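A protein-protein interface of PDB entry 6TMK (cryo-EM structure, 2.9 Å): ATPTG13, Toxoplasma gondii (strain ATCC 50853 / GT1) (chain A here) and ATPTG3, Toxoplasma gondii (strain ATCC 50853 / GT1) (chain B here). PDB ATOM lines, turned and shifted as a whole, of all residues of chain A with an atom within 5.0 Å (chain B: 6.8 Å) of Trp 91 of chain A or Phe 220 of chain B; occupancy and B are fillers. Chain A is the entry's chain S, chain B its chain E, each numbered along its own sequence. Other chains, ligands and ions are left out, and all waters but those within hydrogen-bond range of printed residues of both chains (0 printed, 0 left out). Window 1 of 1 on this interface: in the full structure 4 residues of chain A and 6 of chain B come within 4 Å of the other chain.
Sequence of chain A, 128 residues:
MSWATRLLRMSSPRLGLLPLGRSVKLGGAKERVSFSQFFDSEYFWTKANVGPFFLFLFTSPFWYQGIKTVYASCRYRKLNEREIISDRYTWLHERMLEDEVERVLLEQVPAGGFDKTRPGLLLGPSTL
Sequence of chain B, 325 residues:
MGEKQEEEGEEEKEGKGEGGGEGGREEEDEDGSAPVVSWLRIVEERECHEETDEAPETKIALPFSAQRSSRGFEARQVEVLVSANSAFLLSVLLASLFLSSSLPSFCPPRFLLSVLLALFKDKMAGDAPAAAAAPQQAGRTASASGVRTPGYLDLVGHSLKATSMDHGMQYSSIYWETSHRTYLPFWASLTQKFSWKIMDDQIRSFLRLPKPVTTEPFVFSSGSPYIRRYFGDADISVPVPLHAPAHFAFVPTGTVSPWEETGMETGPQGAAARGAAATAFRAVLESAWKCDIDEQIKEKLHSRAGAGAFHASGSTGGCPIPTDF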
ATOM      1  N   ASP A  87     -23.900  31.254   3.958  1.00  0.00           N
ATOM      2  CA  ASP A  87     -24.977  31.165   2.984  1.00  0.00           C
ATOM      3  C   ASP A  87     -25.032  29.777   2.365  1.00  0.00           C
ATOM      4  O   ASP A  87     -26.121  29.221   2.155  1.00  0.00           O
ATOM      5  CB  ASP A  87     -24.791  32.234   1.912  1.00  0.00           C
ATOM      6  CG  ASP A  87     -25.918  32.255   0.900  1.00  0.00           C
ATOM      7  OD1 ASP A  87     -25.672  31.902  -0.275  1.00  0.00           O
ATOM      8  OD2 ASP A  87     -27.050  32.633   1.277  1.00  0.00           O
ATOM      9  N   ARG A  88     -23.870  29.184   2.092  1.00  0.00           N
ATOM     10  CA  ARG A  88     -23.864  27.846   1.515  1.00  0.00           C
ATOM     11  C   ARG A  88     -24.353  26.797   2.509  1.00  0.00           C
ATOM     12  O   ARG A  88     -25.013  25.831   2.111  1.00  0.00           O
ATOM     13  CB  ARG A  88     -22.474  27.516   1.004  1.00  0.00           C
ATOM     14  CG  ARG A  88     -22.130  28.284  -0.223  1.00  0.00           C
ATOM     15  CD  ARG A  88     -20.772  27.966  -0.737  1.00  0.00           C
ATOM     16  NE  ARG A  88     -20.452  28.759  -1.913  1.00  0.00           N
ATOM     17  CZ  ARG A  88     -19.296  28.699  -2.556  1.00  0.00           C
ATOM     18  NH1 ARG A  88     -18.354  27.878  -2.139  1.00  0.00           N
ATOM     19  NH2 ARG A  88     -19.089  29.455  -3.616  1.00  0.00           N
ATOM     20  N   TYR A  89     -24.062  26.972   3.799  1.00  0.00           N
ATOM     21  CA  TYR A  89     -24.582  26.046   4.800  1.00  0.00           C
ATOM     22  C   TYR A  89     -26.096  26.153   4.916  1.00  0.00           C
ATOM     23  O   TYR A  89     -26.782  25.143   5.100  1.00  0.00           O
ATOM     24  CB  TYR A  89     -23.923  26.296   6.151  1.00  0.00           C
ATOM     25  CG  TYR A  89     -22.687  25.471   6.390  1.00  0.00           C
ATOM     26  CD1 TYR A  89     -22.762  24.095   6.476  1.00  0.00           C
ATOM     27  CD2 TYR A  89     -21.450  26.062   6.533  1.00  0.00           C
ATOM     28  CE1 TYR A  89     -21.646  23.337   6.693  1.00  0.00           C
ATOM     29  CE2 TYR A  89     -20.328  25.309   6.750  1.00  0.00           C
ATOM     30  CZ  TYR A  89     -20.431  23.946   6.829  1.00  0.00           C
ATOM     31  OH  TYR A  89     -19.312  23.184   7.050  1.00  0.00           O
ATOM     32  N   THR A  90     -26.632  27.366   4.816  1.00  0.00           N
ATOM     33  CA  THR A  90     -28.083  27.534   4.837  1.00  0.00           C
ATOM     34  C   THR A  90     -28.721  26.832   3.642  1.00  0.00           C
ATOM     35  O   THR A  90     -29.737  26.128   3.771  1.00  0.00           O
ATOM     36  CB  THR A  90     -28.427  29.020   4.841  1.00  0.00           C
ATOM     37  OG1 THR A  90     -27.768  29.663   5.934  1.00  0.00           O
ATOM     38  CG2 THR A  90     -29.901  29.217   4.986  1.00  0.00           C
ATOM     39  N   TRP A  91     -28.136  27.033   2.462  1.00  0.00           N
ATOM     40  CA  TRP A  91     -28.565  26.319   1.268  1.00  0.00           C
ATOM     41  C   TRP A  91     -28.594  24.812   1.501  1.00  0.00           C
ATOM     42  O   TRP A  91     -29.594  24.139   1.212  1.00  0.00           O
ATOM     43  CB  TRP A  91     -27.619  26.698   0.128  1.00  0.00           C
ATOM     44  CG  TRP A  91     -27.818  25.983  -1.150  1.00  0.00           C
ATOM     45  CD1 TRP A  91     -28.696  26.296  -2.132  1.00  0.00           C
ATOM     46  CD2 TRP A  91     -27.093  24.842  -1.607  1.00  0.00           C
ATOM     47  NE1 TRP A  91     -28.579  25.413  -3.169  1.00  0.00           N
ATOM     48  CE2 TRP A  91     -27.599  24.508  -2.869  1.00  0.00           C
ATOM     49  CE3 TRP A  91     -26.072  24.065  -1.064  1.00  0.00           C
ATOM     50  CZ2 TRP A  91     -27.119  23.432  -3.598  1.00  0.00           C
ATOM     51  CZ3 TRP A  91     -25.600  23.004  -1.785  1.00  0.00           C
ATOM     52  CH2 TRP A  91     -26.120  22.694  -3.039  1.00  0.00           C
ATOM     53  N   LEU A  92     -27.495  24.263   2.018  1.00  0.00           N
ATOM     54  CA  LEU A  92     -27.411  22.828   2.252  1.00  0.00           C
ATOM     55  C   LEU A  92     -28.464  22.354   3.245  1.00  0.00           C
ATOM     56  O   LEU A  92     -29.032  21.269   3.087  1.00  0.00           O
ATOM     57  CB  LEU A  92     -26.019  22.479   2.754  1.00  0.00           C
ATOM     58  CG  LEU A  92     -25.741  21.008   3.011  1.00  0.00           C
ATOM     59  CD1 LEU A  92     -25.828  20.231   1.732  1.00  0.00           C
ATOM     60  CD2 LEU A  92     -24.390  20.873   3.627  1.00  0.00           C
ATOM     61  N   HIS A  93     -28.716  23.142   4.285  1.00  0.00           N
ATOM     62  CA  HIS A  93     -29.744  22.805   5.262  1.00  0.00           C
ATOM     63  C   HIS A  93     -31.098  22.643   4.588  1.00  0.00           C
ATOM     64  O   HIS A  93     -31.805  21.642   4.793  1.00  0.00           O
ATOM     65  CB  HIS A  93     -29.779  23.896   6.328  1.00  0.00           C
ATOM     66  CG  HIS A  93     -30.749  23.647   7.436  1.00  0.00           C
ATOM     67  ND1 HIS A  93     -31.626  24.613   7.881  1.00  0.00           N
ATOM     68  CD2 HIS A  93     -30.968  22.559   8.206  1.00  0.00           C
ATOM     69  CE1 HIS A  93     -32.349  24.123   8.869  1.00  0.00           C
ATOM     70  NE2 HIS A  93     -31.969  22.879   9.087  1.00  0.00           N
ATOM     71  N   GLU A  94     -31.472  23.622   3.769  1.00  0.00           N
ATOM     72  CA  GLU A  94     -32.762  23.556   3.092  1.00  0.00           C
ATOM     73  C   GLU A  94     -32.838  22.352   2.162  1.00  0.00           C
ATOM     74  O   GLU A  94     -33.868  21.665   2.095  1.00  0.00           O
ATOM     75  CB  GLU A  94     -32.996  24.848   2.326  1.00  0.00           C
ATOM     76  CG  GLU A  94     -33.391  25.991   3.211  1.00  0.00           C
ATOM     77  CD  GLU A  94     -32.947  27.332   2.673  1.00  0.00           C
ATOM     78  OE1 GLU A  94     -32.672  27.430   1.459  1.00  0.00           O
ATOM     79  OE2 GLU A  94     -32.869  28.291   3.468  1.00  0.00           O
ATOM     80  N   ARG A  95     -31.751  22.071   1.446  1.00  0.00           N
ATOM     81  CA  ARG A  95     -31.765  20.946   0.519  1.00  0.00           C
ATOM     82  C   ARG A  95     -31.868  19.617   1.259  1.00  0.00           C
ATOM     83  O   ARG A  95     -32.532  18.686   0.790  1.00  0.00           O
ATOM     84  CB  ARG A  95     -30.512  20.982  -0.348  1.00  0.00           C
ATOM     85  CG  ARG A  95     -30.361  22.243  -1.156  1.00  0.00           C
ATOM     86  CD  ARG A  95     -31.371  22.354  -2.274  1.00  0.00           C
ATOM     87  NE  ARG A  95     -32.666  22.868  -1.843  1.00  0.00           N
ATOM     88  CZ  ARG A  95     -32.879  24.108  -1.421  1.00  0.00           C
ATOM     89  NH1 ARG A  95     -34.092  24.484  -1.058  1.00  0.00           N
ATOM     90  NH2 ARG A  95     -31.884  24.969  -1.356  1.00  0.00           N
ATOM     91  N   VAL B 213     -17.333  34.387  -6.376  1.00  0.00           N
ATOM     92  CA  VAL B 213     -18.023  33.122  -6.583  1.00  0.00           C
ATOM     93  C   VAL B 213     -18.442  32.910  -8.025  1.00  0.00           C
ATOM     94  O   VAL B 213     -18.890  31.814  -8.373  1.00  0.00           O
ATOM     95  CB  VAL B 213     -19.252  33.048  -5.658  1.00  0.00           C
ATOM     96  CG1 VAL B 213     -18.851  33.337  -4.237  1.00  0.00           C
ATOM     97  CG2 VAL B 213     -20.307  34.027  -6.101  1.00  0.00           C
ATOM     98  N   GLU B 216     -17.117  29.943  -9.909  1.00  0.00           N
ATOM     99  CA  GLU B 216     -17.719  28.642  -9.715  1.00  0.00           C
ATOM    100  C   GLU B 216     -18.987  28.558 -10.547  1.00  0.00           C
ATOM    101  O   GLU B 216     -19.869  29.414 -10.390  1.00  0.00           O
ATOM    102  CB  GLU B 216     -18.030  28.409  -8.244  1.00  0.00           C
ATOM    103  CG  GLU B 216     -18.043  26.951  -7.847  1.00  0.00           C
ATOM    104  CD  GLU B 216     -19.420  26.344  -7.888  1.00  0.00           C
ATOM    105  OE1 GLU B 216     -20.362  26.986  -7.382  1.00  0.00           O
ATOM    106  OE2 GLU B 216     -19.560  25.225  -8.425  1.00  0.00           O
ATOM    107  N   PHE B 218     -21.536  26.433 -10.495  1.00  0.00           N
ATOM    108  CA  PHE B 218     -22.734  26.154  -9.726  1.00  0.00           C
ATOM    109  C   PHE B 218     -23.161  27.402  -8.962  1.00  0.00           C
ATOM    110  O   PHE B 218     -22.341  28.237  -8.576  1.00  0.00           O
ATOM    111  CB  PHE B 218     -22.498  24.993  -8.767  1.00  0.00           C
ATOM    112  CG  PHE B 218     -23.748  24.280  -8.373  1.00  0.00           C
ATOM    113  CD1 PHE B 218     -24.372  23.412  -9.245  1.00  0.00           C
ATOM    114  CD2 PHE B 218     -24.304  24.484  -7.131  1.00  0.00           C
ATOM    115  CE1 PHE B 218     -25.524  22.765  -8.880  1.00  0.00           C
ATOM    116  CE2 PHE B 218     -25.451  23.842  -6.763  1.00  0.00           C
ATOM    117  CZ  PHE B 218     -26.064  22.978  -7.636  1.00  0.00           C
ATOM    118  N   VAL B 219     -24.465  27.517  -8.745  1.00  0.00           N
ATOM    119  CA  VAL B 219     -25.079  28.703  -8.166  1.00  0.00           C
ATOM    120  C   VAL B 219     -25.852  28.275  -6.929  1.00  0.00           C
ATOM    121  O   VAL B 219     -26.823  27.515  -7.027  1.00  0.00           O
ATOM    122  CB  VAL B 219     -25.995  29.418  -9.172  1.00  0.00           C
ATOM    123  CG1 VAL B 219     -26.759  30.523  -8.503  1.00  0.00           C
ATOM    124  CG2 VAL B 219     -25.196  29.961 -10.329  1.00  0.00           C
ATOM    125  N   PHE B 220     -25.418  28.761  -5.772  1.00  0.00           N
ATOM    126  CA  PHE B 220     -26.060  28.488  -4.497  1.00  0.00           C
ATOM    127  C   PHE B 220     -27.072  29.550  -4.103  1.00  0.00           C
ATOM    128  O   PHE B 220     -27.668  29.449  -3.027  1.00  0.00           O
ATOM    129  CB  PHE B 220     -25.004  28.380  -3.400  1.00  0.00           C
ATOM    130  CG  PHE B 220     -23.929  27.384  -3.687  1.00  0.00           C
ATOM    131  CD1 PHE B 220     -23.996  26.111  -3.177  1.00  0.00           C
ATOM    132  CD2 PHE B 220     -22.841  27.728  -4.456  1.00  0.00           C
ATOM    133  CE1 PHE B 220     -23.009  25.204  -3.435  1.00  0.00           C
ATOM    134  CE2 PHE B 220     -21.854  26.820  -4.711  1.00  0.00           C
ATOM    135  CZ  PHE B 220     -21.940  25.559  -4.204  1.00  0.00           C
ATOM    136  N   SER B 221     -27.276  30.564  -4.934  1.00  0.00           N
ATOM    137  CA  SER B 221     -28.118  31.698  -4.589  1.00  0.00           C
ATOM    138  C   SER B 221     -29.601  31.421  -4.780  1.00  0.00           C
ATOM    139  O   SER B 221     -30.406  32.347  -4.654  1.00  0.00           O
ATOM    140  CB  SER B 221     -27.712  32.915  -5.416  1.00  0.00           C
ATOM    141  OG  SER B 221     -26.479  33.445  -4.968  1.00  0.00           O
ATOM    142  N   SER B 222     -29.983  30.183  -5.083  1.00  0.00           N
ATOM    143  CA  SER B 222     -31.385  29.809  -5.106  1.00  0.00           C
ATOM    144  C   SER B 222     -31.509  28.332  -4.775  1.00  0.00           C
ATOM    145  O   SER B 222     -30.520  27.599  -4.703  1.00  0.00           O
ATOM    146  CB  SER B 222     -32.024  30.104  -6.462  1.00  0.00           C
ATOM    147  OG  SER B 222     -33.418  29.880  -6.425  1.00  0.00           O
ATOM    148  N   GLY B 223     -32.755  27.905  -4.576  1.00  0.00           N
ATOM    149  CA  GLY B 223     -33.016  26.521  -4.241  1.00  0.00           C
ATOM    150  C   GLY B 223     -33.016  25.615  -5.447  1.00  0.00           C
ATOM    151  O   GLY B 223     -32.619  24.451  -5.349  1.00  0.00           O
ATOM    152  N   SER B 224     -33.454  26.121  -6.586  1.00  0.00           N
ATOM    153  CA  SER B 224     -33.474  25.341  -7.805  1.00  0.00           C
ATOM    154  C   SER B 224     -32.110  25.397  -8.492  1.00  0.00           C
ATOM    155  O   SER B 224     -31.379  26.380  -8.355  1.00  0.00           O
ATOM    156  CB  SER B 224     -34.558  25.857  -8.742  1.00  0.00           C
ATOM    157  OG  SER B 224     -34.283  27.170  -9.186  1.00  0.00           O
ATOM    158  N   TYR B 226     -29.110  26.066 -10.789  1.00  0.00           N
ATOM    159  CA  TYR B 226     -28.656  26.978 -11.821  1.00  0.00           C
ATOM    160  C   TYR B 226     -27.190  26.709 -12.124  1.00  0.00           C
ATOM    161  O   TYR B 226     -26.411  26.356 -11.237  1.00  0.00           O
ATOM    162  CB  TYR B 226     -28.826  28.439 -11.394  1.00  0.00           C
ATOM    163  CG  TYR B 226     -30.218  29.005 -11.508  1.00  0.00           C
ATOM    164  CD1 TYR B 226     -30.561  29.830 -12.558  1.00  0.00           C
ATOM    165  CD2 TYR B 226     -31.174  28.755 -10.542  1.00  0.00           C
ATOM    166  CE1 TYR B 226     -31.815  30.363 -12.663  1.00  0.00           C
ATOM    167  CE2 TYR B 226     -32.436  29.288 -10.640  1.00  0.00           C
ATOM    168  CZ  TYR B 226     -32.751  30.093 -11.701  1.00  0.00           C
ATOM    169  OH  TYR B 226     -34.012  30.630 -11.806  1.00  0.00           O
ATOM    170  N   ARG B 228     -23.850  28.433 -14.435  1.00  0.00           N
ATOM    171  CA  ARG B 228     -23.408  29.626 -15.138  1.00  0.00           C
ATOM    172  C   ARG B 228     -22.941  29.291 -16.545  1.00  0.00           C
ATOM    173  O   ARG B 228     -22.230  28.308 -16.768  1.00  0.00           O
ATOM    174  CB  ARG B 228     -22.279  30.318 -14.382  1.00  0.00           C
ATOM    175  CG  ARG B 228     -22.678  30.868 -13.048  1.00  0.00           C
ATOM    176  CD  ARG B 228     -21.498  31.444 -12.320  1.00  0.00           C
ATOM    177  NE  ARG B 228     -21.830  31.839 -10.961  1.00  0.00           N
ATOM    178  CZ  ARG B 228     -22.534  32.917 -10.652  1.00  0.00           C
ATOM    179  NH1 ARG B 228     -22.984  33.716 -11.603  1.00  0.00           N
ATOM    180  NH2 ARG B 228     -22.786  33.195  -9.387  1.00  0.00           N
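The backbone carbonyl oxygen (O) of Ser 222 of chain B lies within hydrogen-bond range of the indole nitrogen (NE1) of Trp 91 of chain A, 3.3 Å away.
NH2 of Arg 95 of chain A is in salt-bridge range of OE1 of Glu 94 of chain A (3.8 Å). The backbone NH (N) of Phe 218 of chain B lies close to the side-chain carboxylate (OE2) of Glu 216 of chain B (3.1 Å).
Val 213 of chain B touches Arg 88 of chain A. Arg 88 of chain A touches Phe 220 of chain B. CZ2 of Trp 91 of chain A touches CE2 of Phe 218 of chain B, at 3.6 Å. Trp 91 of chain A touches Phe 220 of chain B (CD1 to O, 3.4 Å). NH2 of Arg 95 of chain A touches CA of Gly 223 of chain B, 3.5 Å away.
Of chain B, only Phe 218, Phe 220 and Ser 222 come within 4 Å of Trp 91 of chain A. Of chain A, only Arg 88 (3.6 Å) and Trp 91 (3.4 Å) come within 4 Å of Phe 220 of chain B. Of the printed residues of chain B, Arg 95 of chain A touches Gly 223 (3.5 Å). Printed residues of chain A within 4 Å of Gly 223 of chain B: Arg 95. Ser 221 of chain B touches none of the printed residues of chain A. Tyr 89 of chain A touches none of the printed residues of chain B. The nearest residue of chain B that does not touch Trp 91 of chain A is Gly 223 of chain B (4.7 Å).
Printed residues of chain A that touch a printed residue of chain B: Arg 88, Trp 91 and Arg 95. Hydrophobic or aromatic side chains of chain A that line the printed part of chain B: Trp 91. Of the 11 printed residues of chain B, 5 touch a printed residue of chain A.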
